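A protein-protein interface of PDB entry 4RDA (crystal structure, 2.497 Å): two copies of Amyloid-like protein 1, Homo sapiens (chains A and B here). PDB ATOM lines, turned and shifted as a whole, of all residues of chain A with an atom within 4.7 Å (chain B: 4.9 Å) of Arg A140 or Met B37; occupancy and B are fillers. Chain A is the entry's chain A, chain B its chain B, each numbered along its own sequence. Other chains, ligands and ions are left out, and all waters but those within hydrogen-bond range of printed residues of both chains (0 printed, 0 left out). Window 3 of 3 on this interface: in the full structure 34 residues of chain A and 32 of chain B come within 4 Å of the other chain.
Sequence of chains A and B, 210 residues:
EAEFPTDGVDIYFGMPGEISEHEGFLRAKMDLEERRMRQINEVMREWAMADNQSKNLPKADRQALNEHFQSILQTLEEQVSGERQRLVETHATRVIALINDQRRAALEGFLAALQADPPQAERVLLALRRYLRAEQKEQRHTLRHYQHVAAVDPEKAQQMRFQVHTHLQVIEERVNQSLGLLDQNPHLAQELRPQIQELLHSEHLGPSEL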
ATOM      1  N   GLN A 136     -18.813  17.891   4.098  1.00  0.00           N
ATOM      2  CA  GLN A 136     -19.855  16.914   4.392  1.00  0.00           C
ATOM      3  C   GLN A 136     -20.010  16.712   5.908  1.00  0.00           C
ATOM      4  O   GLN A 136     -21.112  16.426   6.411  1.00  0.00           O
ATOM      5  CB  GLN A 136     -19.549  15.591   3.701  1.00  0.00           C
ATOM      6  CG  GLN A 136     -20.736  14.668   3.539  1.00  0.00           C
ATOM      7  CD  GLN A 136     -20.397  13.456   2.675  1.00  0.00           C
ATOM      8  OE1 GLN A 136     -19.624  12.586   3.085  1.00  0.00           O
ATOM      9  NE2 GLN A 136     -20.962  13.404   1.466  1.00  0.00           N
ATOM     10  N   LYS A 137     -18.913  16.875   6.643  1.00  0.00           N
ATOM     11  CA  LYS A 137     -18.999  16.785   8.082  1.00  0.00           C
ATOM     12  C   LYS A 137     -19.857  17.939   8.612  1.00  0.00           C
ATOM     13  O   LYS A 137     -20.639  17.757   9.564  1.00  0.00           O
ATOM     14  CB  LYS A 137     -17.602  16.777   8.734  1.00  0.00           C
ATOM     15  CG  LYS A 137     -17.656  16.694  10.260  1.00  0.00           C
ATOM     16  CD  LYS A 137     -16.272  16.577  10.918  1.00  0.00           C
ATOM     17  CE  LYS A 137     -15.612  15.227  10.628  1.00  0.00           C
ATOM     18  N   GLU A 138     -19.758  19.111   7.984  1.00  0.00           N
ATOM     19  CA  GLU A 138     -20.568  20.234   8.445  1.00  0.00           C
ATOM     20  C   GLU A 138     -22.031  20.022   8.066  1.00  0.00           C
ATOM     21  O   GLU A 138     -22.941  20.376   8.812  1.00  0.00           O
ATOM     22  CB  GLU A 138     -20.079  21.574   7.889  1.00  0.00           C
ATOM     23  CG  GLU A 138     -20.946  22.713   8.412  1.00  0.00           C
ATOM     24  CD  GLU A 138     -20.423  24.081   8.076  1.00  0.00           C
ATOM     25  OE1 GLU A 138     -19.199  24.268   8.120  1.00  0.00           O
ATOM     26  OE2 GLU A 138     -21.238  24.976   7.775  1.00  0.00           O
ATOM     27  N   GLN A 139     -22.255  19.447   6.895  1.00  0.00           N
ATOM     28  CA  GLN A 139     -23.614  19.161   6.464  1.00  0.00           C
ATOM     29  C   GLN A 139     -24.297  18.155   7.402  1.00  0.00           C
ATOM     30  O   GLN A 139     -25.456  18.347   7.766  1.00  0.00           O
ATOM     31  CB  GLN A 139     -23.630  18.640   5.020  1.00  0.00           C
ATOM     32  CG  GLN A 139     -25.004  18.154   4.583  1.00  0.00           C
ATOM     33  CD  GLN A 139     -24.960  17.379   3.304  1.00  0.00           C
ATOM     34  OE1 GLN A 139     -23.895  16.962   2.860  1.00  0.00           O
ATOM     35  NE2 GLN A 139     -26.115  17.190   2.681  1.00  0.00           N
ATOM     36  N   ARG A 140     -23.591  17.091   7.788  1.00  0.00           N
ATOM     37  CA  ARG A 140     -24.178  16.061   8.646  1.00  0.00           C
ATOM     38  C   ARG A 140     -24.407  16.575  10.061  1.00  0.00           C
ATOM     39  O   ARG A 140     -25.404  16.237  10.695  1.00  0.00           O
ATOM     40  CB  ARG A 140     -23.297  14.818   8.676  1.00  0.00           C
ATOM     41  CG  ARG A 140     -23.231  14.131   7.329  1.00  0.00           C
ATOM     42  CD  ARG A 140     -22.360  12.888   7.361  1.00  0.00           C
ATOM     43  NE  ARG A 140     -23.074  11.744   7.922  1.00  0.00           N
ATOM     44  CZ  ARG A 140     -22.855  11.243   9.133  1.00  0.00           C
ATOM     45  N   HIS A 141     -23.492  17.409  10.544  1.00  0.00           N
ATOM     46  CA  HIS A 141     -23.658  18.052  11.833  1.00  0.00           C
ATOM     47  C   HIS A 141     -24.868  18.982  11.830  1.00  0.00           C
ATOM     48  O   HIS A 141     -25.556  19.126  12.835  1.00  0.00           O
ATOM     49  CB  HIS A 141     -22.402  18.831  12.204  1.00  0.00           C
ATOM     50  CG  HIS A 141     -22.413  19.340  13.609  1.00  0.00           C
ATOM     51  ND1 HIS A 141     -22.927  20.570  13.953  1.00  0.00           N
ATOM     52  CD2 HIS A 141     -21.996  18.770  14.763  1.00  0.00           C
ATOM     53  CE1 HIS A 141     -22.819  20.745  15.257  1.00  0.00           C
ATOM     54  NE2 HIS A 141     -22.254  19.667  15.770  1.00  0.00           N
ATOM     55  N   THR A 142     -25.143  19.610  10.698  1.00  0.00           N
ATOM     56  CA  THR A 142     -26.279  20.526  10.607  1.00  0.00           C
ATOM     57  C   THR A 142     -27.593  19.762  10.626  1.00  0.00           C
ATOM     58  O   THR A 142     -28.553  20.185  11.255  1.00  0.00           O
ATOM     59  CB  THR A 142     -26.214  21.381   9.342  1.00  0.00           C
ATOM     60  OG1 THR A 142     -24.996  22.119   9.353  1.00  0.00           O
ATOM     61  CG2 THR A 142     -27.362  22.347   9.298  1.00  0.00           C
ATOM     62  N   LEU A 143     -27.626  18.635   9.932  1.00  0.00           N
ATOM     63  CA  LEU A 143     -28.802  17.776   9.911  1.00  0.00           C
ATOM     64  C   LEU A 143     -29.031  17.083  11.257  1.00  0.00           C
ATOM     65  O   LEU A 143     -30.156  17.026  11.744  1.00  0.00           O
ATOM     66  CB  LEU A 143     -28.668  16.728   8.812  1.00  0.00           C
ATOM     67  CG  LEU A 143     -28.823  17.191   7.371  1.00  0.00           C
ATOM     68  CD1 LEU A 143     -28.548  16.018   6.447  1.00  0.00           C
ATOM     69  CD2 LEU A 143     -30.220  17.735   7.125  1.00  0.00           C
ATOM     70  N   ARG A 144     -27.959  16.560  11.851  1.00  0.00           N
ATOM     71  CA  ARG A 144     -28.058  15.762  13.077  1.00  0.00           C
ATOM     72  C   ARG A 144     -28.464  16.590  14.286  1.00  0.00           C
ATOM     73  O   ARG A 144     -29.283  16.160  15.099  1.00  0.00           O
ATOM     74  CB  ARG A 144     -26.734  15.056  13.369  1.00  0.00           C
ATOM     75  CG  ARG A 144     -26.823  14.094  14.531  1.00  0.00           C
ATOM     76  CD  ARG A 144     -25.471  13.503  14.897  1.00  0.00           C
ATOM     77  NE  ARG A 144     -24.959  12.650  13.840  1.00  0.00           N
ATOM     78  CZ  ARG A 144     -23.912  12.946  13.069  1.00  0.00           C
ATOM     79  NH1 ARG A 144     -23.232  14.085  13.250  1.00  0.00           N
ATOM     80  NH2 ARG A 144     -23.538  12.089  12.120  1.00  0.00           N
ATOM     81  N   GLN A 147     -32.015  17.248  13.875  1.00  0.00           N
ATOM     82  CA  GLN A 147     -32.745  16.017  14.123  1.00  0.00           C
ATOM     83  C   GLN A 147     -32.803  15.749  15.625  1.00  0.00           C
ATOM     84  O   GLN A 147     -33.797  15.259  16.144  1.00  0.00           O
ATOM     85  CB  GLN A 147     -32.073  14.853  13.368  1.00  0.00           C
ATOM     86  CG  GLN A 147     -32.732  13.487  13.520  1.00  0.00           C
ATOM     87  CD  GLN A 147     -32.283  12.731  14.777  1.00  0.00           C
ATOM     88  OE1 GLN A 147     -31.163  12.914  15.272  1.00  0.00           O
ATOM     89  NE2 GLN A 147     -33.165  11.882  15.298  1.00  0.00           N
ATOM     90  N   GLU B  33     -31.801   7.612  13.829  1.00  0.00           N
ATOM     91  CA  GLU B  33     -31.152   8.886  13.567  1.00  0.00           C
ATOM     92  C   GLU B  33     -30.712   9.011  12.091  1.00  0.00           C
ATOM     93  O   GLU B  33     -30.992  10.023  11.450  1.00  0.00           O
ATOM     94  CB  GLU B  33     -29.957   9.068  14.503  1.00  0.00           C
ATOM     95  CG  GLU B  33     -29.117  10.296  14.209  1.00  0.00           C
ATOM     96  CD  GLU B  33     -28.000  10.497  15.214  1.00  0.00           C
ATOM     97  OE1 GLU B  33     -28.310  10.732  16.405  1.00  0.00           O
ATOM     98  OE2 GLU B  33     -26.820  10.430  14.816  1.00  0.00           O
ATOM     99  N   GLU B  34     -30.039   7.988  11.561  1.00  0.00           N
ATOM    100  CA  GLU B  34     -29.593   8.016  10.171  1.00  0.00           C
ATOM    101  C   GLU B  34     -30.800   8.044   9.235  1.00  0.00           C
ATOM    102  O   GLU B  34     -30.806   8.762   8.240  1.00  0.00           O
ATOM    103  CB  GLU B  34     -28.689   6.819   9.835  1.00  0.00           C
ATOM    104  CG  GLU B  34     -27.349   6.758  10.589  1.00  0.00           C
ATOM    105  CD  GLU B  34     -26.356   7.878  10.233  1.00  0.00           C
ATOM    106  OE1 GLU B  34     -26.613   8.672   9.292  1.00  0.00           O
ATOM    107  OE2 GLU B  34     -25.295   7.952  10.905  1.00  0.00           O
ATOM    108  N   ARG B  35     -31.829   7.279   9.579  1.00  0.00           N
ATOM    109  CA  ARG B  35     -33.083   7.256   8.828  1.00  0.00           C
ATOM    110  C   ARG B  35     -33.739   8.645   8.750  1.00  0.00           C
ATOM    111  O   ARG B  35     -34.135   9.081   7.667  1.00  0.00           O
ATOM    112  CB  ARG B  35     -34.033   6.239   9.466  1.00  0.00           C
ATOM    113  CG  ARG B  35     -35.290   5.928   8.702  1.00  0.00           C
ATOM    114  CD  ARG B  35     -36.136   4.918   9.487  1.00  0.00           C
ATOM    115  NE  ARG B  35     -35.438   3.648   9.698  1.00  0.00           N
ATOM    116  CZ  ARG B  35     -35.966   2.584  10.305  1.00  0.00           C
ATOM    117  NH1 ARG B  35     -37.208   2.625  10.781  1.00  0.00           N
ATOM    118  NH2 ARG B  35     -35.245   1.473  10.447  1.00  0.00           N
ATOM    119  N   ARG B  36     -33.818   9.349   9.879  1.00  0.00           N
ATOM    120  CA  ARG B  36     -34.497  10.653   9.932  1.00  0.00           C
ATOM    121  C   ARG B  36     -33.690  11.811   9.326  1.00  0.00           C
ATOM    122  O   ARG B  36     -34.261  12.795   8.869  1.00  0.00           O
ATOM    123  CB  ARG B  36     -34.855  11.009  11.379  1.00  0.00           C
ATOM    124  CG  ARG B  36     -35.886  10.107  12.009  1.00  0.00           C
ATOM    125  CD  ARG B  36     -37.206  10.176  11.271  1.00  0.00           C
ATOM    126  NE  ARG B  36     -38.241   9.430  11.976  1.00  0.00           N
ATOM    127  CZ  ARG B  36     -39.529   9.458  11.650  1.00  0.00           C
ATOM    128  NH1 ARG B  36     -39.940  10.199  10.626  1.00  0.00           N
ATOM    129  NH2 ARG B  36     -40.407   8.754  12.355  1.00  0.00           N
ATOM    130  N   MET B  37     -32.366  11.716   9.359  1.00  0.00           N
ATOM    131  CA  MET B  37     -31.531  12.725   8.733  1.00  0.00           C
ATOM    132  C   MET B  37     -31.748  12.708   7.227  1.00  0.00           C
ATOM    133  O   MET B  37     -31.734  13.754   6.581  1.00  0.00           O
ATOM    134  CB  MET B  37     -30.053  12.500   9.057  1.00  0.00           C
ATOM    135  CG  MET B  37     -29.653  12.919  10.470  1.00  0.00           C
ATOM    136  SD  MET B  37     -28.026  12.287  10.988  1.00  0.00           S
ATOM    137  CE  MET B  37     -26.954  13.072   9.767  1.00  0.00           C
ATOM    138  N   ARG B  38     -31.972  11.527   6.664  1.00  0.00           N
ATOM    139  CA  ARG B  38     -32.164  11.435   5.222  1.00  0.00           C
ATOM    140  C   ARG B  38     -33.512  12.016   4.827  1.00  0.00           C
ATOM    141  O   ARG B  38     -33.611  12.699   3.818  1.00  0.00           O
ATOM    142  CB  ARG B  38     -32.044   9.994   4.728  1.00  0.00           C
ATOM    143  CG  ARG B  38     -30.628   9.468   4.698  1.00  0.00           C
ATOM    144  CD  ARG B  38     -30.551   8.098   4.019  1.00  0.00           C
ATOM    145  NE  ARG B  38     -30.230   7.022   4.964  1.00  0.00           N
ATOM    146  CZ  ARG B  38     -31.125   6.213   5.533  1.00  0.00           C
ATOM    147  NH1 ARG B  38     -32.420   6.334   5.255  1.00  0.00           N
ATOM    148  NH2 ARG B  38     -30.721   5.269   6.379  1.00  0.00           N
ATOM    149  N   GLN B  39     -34.550  11.753   5.615  1.00  0.00           N
ATOM    150  CA  GLN B  39     -35.861  12.347   5.340  1.00  0.00           C
ATOM    151  C   GLN B  39     -35.770  13.857   5.352  1.00  0.00           C
ATOM    152  O   GLN B  39     -36.272  14.542   4.458  1.00  0.00           O
ATOM    153  CB  GLN B  39     -36.902  11.910   6.361  1.00  0.00           C
ATOM    154  CG  GLN B  39     -37.298  10.457   6.299  1.00  0.00           C
ATOM    155  CD  GLN B  39     -38.374  10.147   7.307  1.00  0.00           C
ATOM    156  OE1 GLN B  39     -39.137  11.028   7.691  1.00  0.00           O
ATOM    157  NE2 GLN B  39     -38.430   8.897   7.760  1.00  0.00           N
ATOM    158  N   ILE B  40     -35.122  14.373   6.383  1.00  0.00           N
ATOM    159  CA  ILE B  40     -34.997  15.805   6.527  1.00  0.00           C
ATOM    160  C   ILE B  40     -34.174  16.384   5.384  1.00  0.00           C
ATOM    161  O   ILE B  40     -34.507  17.434   4.860  1.00  0.00           O
ATOM    162  CB  ILE B  40     -34.376  16.175   7.876  1.00  0.00           C
ATOM    163  CG1 ILE B  40     -35.245  15.638   9.006  1.00  0.00           C
ATOM    164  CG2 ILE B  40     -34.218  17.689   7.996  1.00  0.00           C
ATOM    165  CD1 ILE B  40     -34.652  15.849  10.382  1.00  0.00           C
ATOM    166  N   ASN B  41     -33.112  15.705   4.980  1.00  0.00           N
ATOM    167  CA  ASN B  41     -32.309  16.235   3.881  1.00  0.00           C
ATOM    168  C   ASN B  41     -33.117  16.264   2.598  1.00  0.00           C
ATOM    169  O   ASN B  41     -33.039  17.237   1.868  1.00  0.00           O
ATOM    170  CB  ASN B  41     -31.020  15.440   3.677  1.00  0.00           C
ATOM    171  CG  ASN B  41     -29.967  16.228   2.900  1.00  0.00           C
ATOM    172  OD1 ASN B  41     -30.032  17.459   2.795  1.00  0.00           O
ATOM    173  ND2 ASN B  41     -28.987  15.519   2.356  1.00  0.00           N
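The side-chain amide nitrogen (NE2) of Gln A139 lies close to the side-chain amide nitrogen (ND2) of Asn B41 (3.3 Å). OE2 of Glu B33 is in salt-bridge range of NE of Arg A144 (3.1 Å).
The side-chain amide oxygen of Gln B39 lies within hydrogen-bond range of the guanidinium group of Arg B36, at 3.2 Å.
Among the printed residues, pairs that only touch across the chains: Gln A147 with Glu B33, Arg A140 with Met B37, Leu A143 with Asn B41, Arg A144 with Met B37, Gln A147 with Arg B36 and Leu A143 with Met B37.
Of the printed residues of chain B, Gln A139 touches Asn B41 (3.3 Å). Printed residues of chain B within 4 Å of Arg A140: Met B37 (3.6 Å). His A141 touches none of the printed residues of chain B. Printed residues of chain B within 4 Å of Gln A147: Glu B33 and Arg B36. Printed residues of chain A within 4 Å of Arg B36: Gln A147 (3.9 Å). Of chain A, only Arg A140 (3.6 Å), Leu A143 (3.9 Å) and Arg A144 (3.9 Å) come within 4 Å of Met B37. Ile B40 touches none of the printed residues of chain A. Of the printed residues of chain A, Asn B41 touches Gln A139 (3.3 Å) and Leu A143 (3.8 Å). The nearest residue of chain A that does not touch Met B37 is Gln A147 (4.2 Å). The nearest printed residue of chain A that does not touch Glu B33 is Arg A140 (7.0 Å).
Of the 9 printed residues of chain B, 4 touch a printed residue of chain A. Among the printed residues, Asp or Glu carboxylates within 4 Å of a Lys or Arg side-chain nitrogen of the other chain: Arg A144 with Glu B33.
No position is printed for both chains.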
